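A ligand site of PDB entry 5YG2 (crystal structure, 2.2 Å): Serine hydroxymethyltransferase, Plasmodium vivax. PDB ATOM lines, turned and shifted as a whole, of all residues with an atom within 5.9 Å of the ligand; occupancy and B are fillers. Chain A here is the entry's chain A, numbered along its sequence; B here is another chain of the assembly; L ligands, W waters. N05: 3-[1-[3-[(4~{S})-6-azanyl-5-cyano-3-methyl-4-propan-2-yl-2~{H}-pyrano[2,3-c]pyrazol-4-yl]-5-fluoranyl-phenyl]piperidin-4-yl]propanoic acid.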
ATOM      1  N   HIS A 123     -11.605   3.346  33.242  1.00  0.00           N
ATOM      2  CA  HIS A 123     -12.138   2.014  33.010  1.00  0.00           C
ATOM      3  C   HIS A 123     -11.290   1.310  31.941  1.00  0.00           C
ATOM      4  O   HIS A 123     -10.720   1.967  31.056  1.00  0.00           O
ATOM      5  CB  HIS A 123     -13.611   2.116  32.601  1.00  0.00           C
ATOM      6  CG  HIS A 123     -14.390   0.869  32.832  1.00  0.00           C
ATOM      7  ND1 HIS A 123     -14.243  -0.240  32.048  1.00  0.00           N
ATOM      8  CD2 HIS A 123     -15.311   0.560  33.762  1.00  0.00           C
ATOM      9  CE1 HIS A 123     -15.035  -1.199  32.477  1.00  0.00           C
ATOM     10  NE2 HIS A 123     -15.698  -0.738  33.519  1.00  0.00           N
ATOM     11  N   LEU A 124     -11.184  -0.009  32.032  1.00  0.00           N
ATOM     12  CA  LEU A 124     -10.394  -0.791  31.078  1.00  0.00           C
ATOM     13  C   LEU A 124     -10.911  -0.637  29.657  1.00  0.00           C
ATOM     14  O   LEU A 124     -10.146  -0.294  28.763  1.00  0.00           O
ATOM     15  CB  LEU A 124     -10.378  -2.275  31.469  1.00  0.00           C
ATOM     16  CG  LEU A 124      -9.593  -3.258  30.582  1.00  0.00           C
ATOM     17  CD1 LEU A 124      -8.137  -3.366  30.999  1.00  0.00           C
ATOM     18  CD2 LEU A 124     -10.225  -4.647  30.632  1.00  0.00           C
ATOM     19  N   CYS A 125     -12.202  -0.910  29.458  1.00  0.00           N
ATOM     20  CA  CYS A 125     -12.973  -0.621  28.207  1.00  0.00           C
ATOM     21  C   CYS A 125     -12.817   0.780  27.584  1.00  0.00           C
ATOM     22  O   CYS A 125     -12.969   0.937  26.367  1.00  0.00           O
ATOM     23  CB  CYS A 125     -14.463  -0.870  28.453  1.00  0.00           C
ATOM     24  SG  CYS A 125     -14.856  -2.578  28.972  1.00  0.00           S
ATOM     25  N   SER A 126     -12.517   1.788  28.406  1.00  0.00           N
ATOM     26  CA  SER A 126     -12.281   3.163  27.932  1.00  0.00           C
ATOM     27  C   SER A 126     -10.810   3.494  27.725  1.00  0.00           C
ATOM     28  O   SER A 126     -10.478   4.627  27.330  1.00  0.00           O
ATOM     29  CB  SER A 126     -12.878   4.150  28.926  1.00  0.00           C
ATOM     30  OG  SER A 126     -14.274   3.977  28.989  1.00  0.00           O
ATOM     31  N   GLY A 127      -9.928   2.535  28.017  1.00  0.00           N
ATOM     32  CA  GLY A 127      -8.505   2.686  27.754  1.00  0.00           C
ATOM     33  C   GLY A 127      -7.577   2.700  28.967  1.00  0.00           C
ATOM     34  O   GLY A 127      -6.373   2.845  28.799  1.00  0.00           O
ATOM     35  N   GLY A 128      -8.138   2.531  30.165  1.00  0.00           N
ATOM     36  CA  GLY A 128      -7.345   2.382  31.368  1.00  0.00           C
ATOM     37  C   GLY A 128      -6.699   1.003  31.455  1.00  0.00           C
ATOM     38  O   GLY A 128      -7.012   0.116  30.667  1.00  0.00           O
ATOM     39  N   HIS A 129      -5.750   0.858  32.384  1.00  0.00           N
ATOM     40  CA  HIS A 129      -5.089  -0.406  32.605  1.00  0.00           C
ATOM     41  C   HIS A 129      -5.800  -1.203  33.678  1.00  0.00           C
ATOM     42  O   HIS A 129      -6.518  -0.647  34.503  1.00  0.00           O
ATOM     43  CB  HIS A 129      -3.628  -0.211  32.981  1.00  0.00           C
ATOM     44  CG  HIS A 129      -2.783  -1.431  32.797  1.00  0.00           C
ATOM     45  ND1 HIS A 129      -2.193  -2.086  33.852  1.00  0.00           N
ATOM     46  CD2 HIS A 129      -2.470  -2.155  31.689  1.00  0.00           C
ATOM     47  CE1 HIS A 129      -1.539  -3.148  33.407  1.00  0.00           C
ATOM     48  NE2 HIS A 129      -1.690  -3.202  32.093  1.00  0.00           N
ATOM     49  N   LEU A 130      -5.571  -2.503  33.653  1.00  0.00           N
ATOM     50  CA  LEU A 130      -6.017  -3.402  34.723  1.00  0.00           C
ATOM     51  C   LEU A 130      -5.623  -2.918  36.119  1.00  0.00           C
ATOM     52  O   LEU A 130      -6.453  -2.902  37.031  1.00  0.00           O
ATOM     53  CB  LEU A 130      -5.407  -4.788  34.512  1.00  0.00           C
ATOM     54  CG  LEU A 130      -5.949  -5.604  33.322  1.00  0.00           C
ATOM     55  CD1 LEU A 130      -5.011  -6.748  33.025  1.00  0.00           C
ATOM     56  CD2 LEU A 130      -7.322  -6.173  33.638  1.00  0.00           C
ATOM     57  N   PHE A 134      -9.283  -2.021  37.819  1.00  0.00           N
ATOM     58  CA  PHE A 134     -10.264  -2.723  37.025  1.00  0.00           C
ATOM     59  C   PHE A 134     -11.021  -3.818  37.770  1.00  0.00           C
ATOM     60  O   PHE A 134     -10.409  -4.734  38.350  1.00  0.00           O
ATOM     61  CB  PHE A 134      -9.690  -3.348  35.758  1.00  0.00           C
ATOM     62  CG  PHE A 134     -10.741  -4.012  34.941  1.00  0.00           C
ATOM     63  CD1 PHE A 134     -11.770  -3.262  34.365  1.00  0.00           C
ATOM     64  CD2 PHE A 134     -10.777  -5.396  34.838  1.00  0.00           C
ATOM     65  CE1 PHE A 134     -12.784  -3.868  33.643  1.00  0.00           C
ATOM     66  CE2 PHE A 134     -11.803  -6.013  34.131  1.00  0.00           C
ATOM     67  CZ  PHE A 134     -12.794  -5.245  33.527  1.00  0.00           C
ATOM     68  N   ASP A 136     -15.317  -5.808  37.382  1.00  0.00           N
ATOM     69  CA  ASP A 136     -16.577  -5.911  36.621  1.00  0.00           C
ATOM     70  C   ASP A 136     -17.629  -6.582  37.531  1.00  0.00           C
ATOM     71  O   ASP A 136     -17.274  -7.327  38.444  1.00  0.00           O
ATOM     72  CB  ASP A 136     -16.330  -6.625  35.261  1.00  0.00           C
ATOM     73  CG  ASP A 136     -16.812  -8.081  35.218  1.00  0.00           C
ATOM     74  OD1 ASP A 136     -17.832  -8.340  34.532  1.00  0.00           O
ATOM     75  OD2 ASP A 136     -16.182  -8.961  35.836  1.00  0.00           O
ATOM     76  N   LYS A 139     -16.713  -9.908  39.054  1.00  0.00           N
ATOM     77  CA  LYS A 139     -15.491 -10.082  39.855  1.00  0.00           C
ATOM     78  C   LYS A 139     -14.600  -8.849  39.992  1.00  0.00           C
ATOM     79  O   LYS A 139     -14.532  -7.992  39.119  1.00  0.00           O
ATOM     80  CB  LYS A 139     -14.651 -11.241  39.271  1.00  0.00           C
ATOM     81  CG  LYS A 139     -14.591 -12.482  40.164  1.00  0.00           C
ATOM     82  CD  LYS A 139     -13.629 -13.525  39.626  1.00  0.00           C
ATOM     83  CE  LYS A 139     -12.165 -13.143  39.776  1.00  0.00           C
ATOM     84  NZ  LYS A 139     -11.743 -12.861  41.187  1.00  0.00           N
ATOM     85  N   VAL A 141     -11.495  -8.164  39.257  1.00  0.00           N
ATOM     86  CA  VAL A 141     -10.544  -8.758  38.313  1.00  0.00           C
ATOM     87  C   VAL A 141      -9.097  -8.396  38.655  1.00  0.00           C
ATOM     88  O   VAL A 141      -8.216  -9.248  38.658  1.00  0.00           O
ATOM     89  CB  VAL A 141     -10.897  -8.312  36.856  1.00  0.00           C
ATOM     90  CG1 VAL A 141      -9.841  -8.744  35.834  1.00  0.00           C
ATOM     91  CG2 VAL A 141     -12.248  -8.869  36.431  1.00  0.00           C
ATOM     92  N   THR A 183      -3.617   2.939  28.781  1.00  0.00           N
ATOM     93  CA  THR A 183      -3.066   1.853  27.936  1.00  0.00           C
ATOM     94  C   THR A 183      -3.441   1.996  26.464  1.00  0.00           C
ATOM     95  O   THR A 183      -2.593   1.764  25.606  1.00  0.00           O
ATOM     96  CB  THR A 183      -3.215   0.435  28.513  1.00  0.00           C
ATOM     97  OG1 THR A 183      -3.782  -0.469  27.546  1.00  0.00           O
ATOM     98  CG2 THR A 183      -4.012   0.417  29.712  1.00  0.00           C
ATOM     99  N   SER A 184      -4.652   2.431  26.158  1.00  0.00           N
ATOM    100  CA  SER A 184      -5.029   2.699  24.769  1.00  0.00           C
ATOM    101  C   SER A 184      -5.800   4.001  24.705  1.00  0.00           C
ATOM    102  O   SER A 184      -7.006   4.021  24.553  1.00  0.00           O
ATOM    103  CB  SER A 184      -5.824   1.518  24.195  1.00  0.00           C
ATOM    104  OG  SER A 184      -6.876   1.172  25.068  1.00  0.00           O
ATOM    105  N   ASN A 354      -3.539  -5.762  18.258  1.00  0.00           N
ATOM    106  CA  ASN A 354      -4.445  -6.344  19.221  1.00  0.00           C
ATOM    107  C   ASN A 354      -5.836  -5.788  19.106  1.00  0.00           C
ATOM    108  O   ASN A 354      -6.053  -4.669  18.645  1.00  0.00           O
ATOM    109  CB  ASN A 354      -3.889  -6.273  20.664  1.00  0.00           C
ATOM    110  CG  ASN A 354      -3.675  -4.866  21.154  1.00  0.00           C
ATOM    111  OD1 ASN A 354      -2.581  -4.335  21.051  1.00  0.00           O
ATOM    112  ND2 ASN A 354      -4.716  -4.250  21.664  1.00  0.00           N
ATOM    113  N   LYS A 355      -6.794  -6.609  19.505  1.00  0.00           N
ATOM    114  CA  LYS A 355      -8.162  -6.206  19.621  1.00  0.00           C
ATOM    115  C   LYS A 355      -8.293  -5.217  20.787  1.00  0.00           C
ATOM    116  O   LYS A 355      -7.525  -5.284  21.756  1.00  0.00           O
ATOM    117  CB  LYS A 355      -9.097  -7.425  19.788  1.00  0.00           C
ATOM    118  CG  LYS A 355      -8.882  -8.274  21.036  1.00  0.00           C
ATOM    119  CD  LYS A 355     -10.072  -9.203  21.264  1.00  0.00           C
ATOM    120  CE  LYS A 355     -10.076  -9.831  22.644  1.00  0.00           C
ATOM    121  NZ  LYS A 355      -9.213 -11.046  22.742  1.00  0.00           N
ATOM    122  N   ASN A 356      -9.248  -4.316  20.688  1.00  0.00           N
ATOM    123  CA  ASN A 356      -9.311  -3.191  21.633  1.00  0.00           C
ATOM    124  C   ASN A 356     -10.711  -2.624  21.628  1.00  0.00           C
ATOM    125  O   ASN A 356     -11.310  -2.416  20.578  1.00  0.00           O
ATOM    126  CB  ASN A 356      -8.295  -2.118  21.218  1.00  0.00           C
ATOM    127  CG  ASN A 356      -7.794  -1.288  22.405  1.00  0.00           C
ATOM    128  OD1 ASN A 356      -6.755  -1.594  22.999  1.00  0.00           O
ATOM    129  ND2 ASN A 356      -8.527  -0.263  22.757  1.00  0.00           N
ATOM    130  N   THR A 357     -11.227  -2.354  22.817  1.00  0.00           N
ATOM    131  CA  THR A 357     -12.537  -1.731  22.966  1.00  0.00           C
ATOM    132  C   THR A 357     -12.613  -0.319  22.376  1.00  0.00           C
ATOM    133  O   THR A 357     -11.590   0.327  22.134  1.00  0.00           O
ATOM    134  CB  THR A 357     -12.891  -1.627  24.446  1.00  0.00           C
ATOM    135  OG1 THR A 357     -11.772  -1.081  25.152  1.00  0.00           O
ATOM    136  CG2 THR A 357     -13.199  -3.004  25.010  1.00  0.00           C
ATOM    137  N   CYS A 364     -16.510  -5.473  27.774  1.00  0.00           N
ATOM    138  CA  CYS A 364     -15.180  -5.819  27.210  1.00  0.00           C
ATOM    139  C   CYS A 364     -15.221  -7.151  26.411  1.00  0.00           C
ATOM    140  O   CYS A 364     -14.169  -7.648  25.958  1.00  0.00           O
ATOM    141  CB  CYS A 364     -14.132  -5.884  28.329  1.00  0.00           C
ATOM    142  SG  CYS A 364     -12.637  -4.945  27.948  1.00  0.00           S
ATOM    143  N   PRO A 367     -14.819  -6.809  21.588  1.00  0.00           N
ATOM    144  CA  PRO A 367     -14.449  -5.400  21.319  1.00  0.00           C
ATOM    145  C   PRO A 367     -14.471  -5.049  19.833  1.00  0.00           C
ATOM    146  O   PRO A 367     -14.152  -5.889  18.991  1.00  0.00           O
ATOM    147  CB  PRO A 367     -13.015  -5.293  21.864  1.00  0.00           C
ATOM    148  CG  PRO A 367     -12.490  -6.675  21.771  1.00  0.00           C
ATOM    149  CD  PRO A 367     -13.658  -7.577  22.086  1.00  0.00           C
ATOM    150  N   ARG A 371      -6.068  -1.823  18.102  1.00  0.00           N
ATOM    151  CA  ARG A 371      -5.119  -0.834  18.427  1.00  0.00           C
ATOM    152  C   ARG A 371      -3.857  -1.161  17.688  1.00  0.00           C
ATOM    153  O   ARG A 371      -3.414  -2.329  17.668  1.00  0.00           O
ATOM    154  CB  ARG A 371      -4.886  -0.883  19.935  1.00  0.00           C
ATOM    155  CG  ARG A 371      -3.976   0.196  20.485  1.00  0.00           C
ATOM    156  CD  ARG A 371      -3.658  -0.105  21.921  1.00  0.00           C
ATOM    157  NE  ARG A 371      -2.732  -1.225  22.023  1.00  0.00           N
ATOM    158  CZ  ARG A 371      -2.082  -1.599  23.109  1.00  0.00           C
ATOM    159  NH1 ARG A 371      -2.228  -0.947  24.274  1.00  0.00           N
ATOM    160  NH2 ARG A 371      -1.273  -2.644  23.023  1.00  0.00           N
ATOM    161  N   GLU B  56       0.297 -11.605  27.280  1.00  0.00           N
ATOM    162  CA  GLU B  56      -0.644 -11.691  28.397  1.00  0.00           C
ATOM    163  C   GLU B  56      -1.637 -12.832  28.281  1.00  0.00           C
ATOM    164  O   GLU B  56      -2.142 -13.119  27.201  1.00  0.00           O
ATOM    165  CB  GLU B  56      -1.403 -10.392  28.573  1.00  0.00           C
ATOM    166  CG  GLU B  56      -0.561  -9.298  29.207  1.00  0.00           C
ATOM    167  CD  GLU B  56      -1.306  -7.994  29.321  1.00  0.00           C
ATOM    168  OE1 GLU B  56      -1.058  -7.102  28.509  1.00  0.00           O
ATOM    169  OE2 GLU B  56      -2.180  -7.861  30.201  1.00  0.00           O
ATOM    170  N   TYR B  63      -4.151 -13.107  24.727  1.00  0.00           N
ATOM    171  CA  TYR B  63      -4.933 -11.918  24.418  1.00  0.00           C
ATOM    172  C   TYR B  63      -4.573 -11.494  23.029  1.00  0.00           C
ATOM    173  O   TYR B  63      -5.471 -11.148  22.251  1.00  0.00           O
ATOM    174  CB  TYR B  63      -4.809 -10.817  25.492  1.00  0.00           C
ATOM    175  CG  TYR B  63      -5.832 -11.111  26.559  1.00  0.00           C
ATOM    176  CD1 TYR B  63      -5.558 -12.020  27.574  1.00  0.00           C
ATOM    177  CD2 TYR B  63      -7.121 -10.592  26.486  1.00  0.00           C
ATOM    178  CE1 TYR B  63      -6.509 -12.354  28.522  1.00  0.00           C
ATOM    179  CE2 TYR B  63      -8.085 -10.932  27.426  1.00  0.00           C
ATOM    180  CZ  TYR B  63      -7.763 -11.807  28.444  1.00  0.00           C
ATOM    181  OH  TYR B  63      -8.690 -12.161  29.403  1.00  0.00           O
ATOM    182  N   TYR B  64      -3.287 -11.552  22.698  1.00  0.00           N
ATOM    183  CA  TYR B  64      -2.855 -11.315  21.303  1.00  0.00           C
ATOM    184  C   TYR B  64      -2.466 -12.611  20.627  1.00  0.00           C
ATOM    185  O   TYR B  64      -2.254 -13.625  21.271  1.00  0.00           O
ATOM    186  CB  TYR B  64      -1.675 -10.342  21.206  1.00  0.00           C
ATOM    187  CG  TYR B  64      -1.642  -9.266  22.245  1.00  0.00           C
ATOM    188  CD1 TYR B  64      -2.807  -8.731  22.802  1.00  0.00           C
ATOM    189  CD2 TYR B  64      -0.415  -8.746  22.651  1.00  0.00           C
ATOM    190  CE1 TYR B  64      -2.737  -7.736  23.763  1.00  0.00           C
ATOM    191  CE2 TYR B  64      -0.347  -7.738  23.593  1.00  0.00           C
ATOM    192  CZ  TYR B  64      -1.496  -7.243  24.155  1.00  0.00           C
ATOM    193  OH  TYR B  64      -1.383  -6.245  25.114  1.00  0.00           O
ATOM    194  N   SER B 263      -5.490 -17.211  37.685  1.00  0.00           N
ATOM    195  CA  SER B 263      -6.170 -15.934  37.624  1.00  0.00           C
ATOM    196  C   SER B 263      -5.509 -14.989  38.622  1.00  0.00           C
ATOM    197  O   SER B 263      -5.441 -13.798  38.368  1.00  0.00           O
ATOM    198  CB  SER B 263      -7.704 -16.050  37.850  1.00  0.00           C
ATOM    199  OG  SER B 263      -8.092 -15.853  39.206  1.00  0.00           O
ATOM    200  N   PHE B 266      -2.258 -13.938  36.762  1.00  0.00           N
ATOM    201  CA  PHE B 266      -2.801 -12.966  35.810  1.00  0.00           C
ATOM    202  C   PHE B 266      -4.304 -13.191  35.639  1.00  0.00           C
ATOM    203  O   PHE B 266      -4.697 -14.323  35.453  1.00  0.00           O
ATOM    204  CB  PHE B 266      -2.129 -13.111  34.455  1.00  0.00           C
ATOM    205  CG  PHE B 266      -2.799 -12.347  33.360  1.00  0.00           C
ATOM    206  CD1 PHE B 266      -2.472 -11.010  33.144  1.00  0.00           C
ATOM    207  CD2 PHE B 266      -3.786 -12.937  32.560  1.00  0.00           C
ATOM    208  CE1 PHE B 266      -3.090 -10.280  32.156  1.00  0.00           C
ATOM    209  CE2 PHE B 266      -4.408 -12.211  31.559  1.00  0.00           C
ATOM    210  CZ  PHE B 266      -4.049 -10.890  31.351  1.00  0.00           C
ATOM    211  N   PRO B 267      -5.140 -12.160  35.638  1.00  0.00           N
ATOM    212  CA  PRO B 267      -4.747 -10.758  35.653  1.00  0.00           C
ATOM    213  C   PRO B 267      -4.853 -10.055  37.032  1.00  0.00           C
ATOM    214  O   PRO B 267      -4.805  -8.808  37.090  1.00  0.00           O
ATOM    215  CB  PRO B 267      -5.757 -10.144  34.685  1.00  0.00           C
ATOM    216  CG  PRO B 267      -7.000 -10.883  35.006  1.00  0.00           C
ATOM    217  CD  PRO B 267      -6.581 -12.294  35.370  1.00  0.00           C
HETATM  218  O33 N05 L   1      -9.908 -12.932  34.257  1.00  0.00           O
HETATM  219  C31 N05 L   1     -10.729 -12.190  33.697  1.00  0.00           C
HETATM  220  O32 N05 L   1     -11.860 -11.957  34.185  1.00  0.00           O
HETATM  221  C30 N05 L   1     -10.322 -11.569  32.376  1.00  0.00           C
HETATM  222  C29 N05 L   1     -10.872 -10.146  32.207  1.00  0.00           C
HETATM  223  C26 N05 L   1     -10.352  -9.533  30.899  1.00  0.00           C
HETATM  224  C25 N05 L   1     -11.382  -8.673  30.230  1.00  0.00           C
HETATM  225  C24 N05 L   1     -10.929  -8.344  28.825  1.00  0.00           C
HETATM  226  C27 N05 L   1      -9.102  -8.726  31.144  1.00  0.00           C
HETATM  227  C28 N05 L   1      -8.449  -8.386  29.800  1.00  0.00           C
HETATM  228  N23 N05 L   1      -9.496  -7.956  28.820  1.00  0.00           N
HETATM  229  C19 N05 L   1      -9.055  -7.198  27.689  1.00  0.00           C
HETATM  230  C34 N05 L   1      -9.652  -7.430  26.433  1.00  0.00           C
HETATM  231  C18 N05 L   1      -9.221  -6.728  25.315  1.00  0.00           C
HETATM  232  F21 N05 L   1      -9.819  -6.934  24.146  1.00  0.00           F
HETATM  233  C17 N05 L   1      -8.206  -5.793  25.379  1.00  0.00           C
HETATM  234  C20 N05 L   1      -8.019  -6.241  27.739  1.00  0.00           C
HETATM  235  C16 N05 L   1      -7.568  -5.534  26.596  1.00  0.00           C
HETATM  236  C4  N05 L   1      -6.465  -4.470  26.667  1.00  0.00           C
HETATM  237  C14 N05 L   1      -5.594  -4.286  25.401  1.00  0.00           C
HETATM  238  C22 N05 L   1      -4.560  -3.131  25.442  1.00  0.00           C
HETATM  239  C15 N05 L   1      -4.886  -5.557  24.947  1.00  0.00           C
HETATM  240  C3  N05 L   1      -7.185  -3.130  26.856  1.00  0.00           C
HETATM  241  C8  N05 L   1      -8.151  -2.883  26.061  1.00  0.00           C
HETATM  242  N9  N05 L   1      -9.032  -2.638  25.343  1.00  0.00           N
HETATM  243  C2  N05 L   1      -6.815  -2.237  27.816  1.00  0.00           C
HETATM  244  N7  N05 L   1      -7.411  -1.071  27.997  1.00  0.00           N
HETATM  245  C5  N05 L   1      -5.565  -4.741  27.840  1.00  0.00           C
HETATM  246  C10 N05 L   1      -4.822  -5.934  28.354  1.00  0.00           C
HETATM  247  C13 N05 L   1      -4.740  -7.333  27.786  1.00  0.00           C
HETATM  248  N11 N05 L   1      -4.209  -5.529  29.476  1.00  0.00           N
HETATM  249  N12 N05 L   1      -4.433  -4.184  29.832  1.00  0.00           N
HETATM  250  C6  N05 L   1      -5.223  -3.752  28.854  1.00  0.00           C
HETATM  251  O1  N05 L   1      -5.709  -2.498  28.725  1.00  0.00           O
HETATM  252  O   HOH W   1      -9.182 -15.502  34.854  1.00  0.00           O
HETATM  253  O   HOH W   2     -10.190 -13.594  36.890  1.00  0.00           O
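C of Gly 127 touches N7 of the ligand, at 3.9 Å. CD2 of His 129 touches N12 of the ligand, 3.4 Å away. Leu 130 touches the ligand. CG2 of Val 141 touches O32 of the ligand, at 3.8 Å. OG of Ser 184 touches N7 of the ligand (3.7 Å). Asn 354 touches the ligand. Lys 355 touches the ligand. Cys 364 touches the ligand. Pro 367 touches the ligand (CG to F21, 3.6 Å). NH1 of Arg 371 touches C22 of the ligand, 3.4 Å away. OH of Tyr 63 of chain B touches C30 of the ligand (3.4 Å). Tyr 64 of chain B touches the ligand (CE1 to C15, 3.3 Å). Pro 267 of chain B touches the ligand. Hydrophobic or aromatic side chains within 4 Å of the ligand: Leu 124, His 129, Leu 130, Val 141, Pro 367, Tyr 63 of chain B, Tyr 64 of chain B and Pro 267 of chain B. 19 residues have an atom within 4 Å of the ligand: Leu 124, Gly 127, Gly 128, His 129, Leu 130, Val 141, Thr 183, Ser 184, Asn 354, Lys 355, Asn 356, Thr 357, Cys 364, Pro 367, Arg 371, Glu 56 of chain B, Tyr 63 of chain B, Tyr 64 of chain B and Pro 267 of chain B.
O of Leu 124 is in hydrogen-bond range of N7 of the ligand. O of Gly 128 is in hydrogen-bond range of N7 of the ligand (2.9 Å). O1 of the ligand sits at hydrogen-bond distance from OG1 of Thr 183. N of Thr 357 sits at hydrogen-bond distance from N9 of the ligand (3.4 Å). The side-chain hydroxyl (OG1) of Thr 357 sits at hydrogen-bond distance from a nitrogen (N9) of the ligand. The side-chain carboxylate (OE2) of Glu 56 of chain B lies within hydrogen-bond range of a nitrogen (N11) of the ligand, at 3.2 Å. The side-chain amide oxygen (OD1) of Asn 356 lies close to a nitrogen (N9) of the ligand, at 3.4 Å.
O of His 123 lies within hydrogen-bond range of N of Gly 128. The guanidinium group (NH1) of Arg 371 is in hydrogen-bond range of the backbone carbonyl oxygen (O) of Thr 183 (3.0 Å). The backbone carbonyl oxygen of Cys 125 lies within hydrogen-bond range of the side-chain hydroxyl of Thr 357, 2.6 Å away. The backbone NH of Tyr 63 of chain B lies within hydrogen-bond range of the backbone carbonyl oxygen of Glu 56 of chain B (3.2 Å). The backbone carbonyl oxygen of Asn 354 sits at hydrogen-bond distance from the backbone NH of Arg 371 (2.9 Å). The side-chain hydroxyl of Ser 184 lies within hydrogen-bond range of the side-chain amide nitrogen of Asn 356 (3.2 Å). The backbone NH (N) of Ser 184 is in hydrogen-bond range of the backbone carbonyl oxygen (O) of Gly 127, at 3.2 Å. SG of Cys 125 is in hydrogen-bond range of SG of Cys 364, 3.4 Å away.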
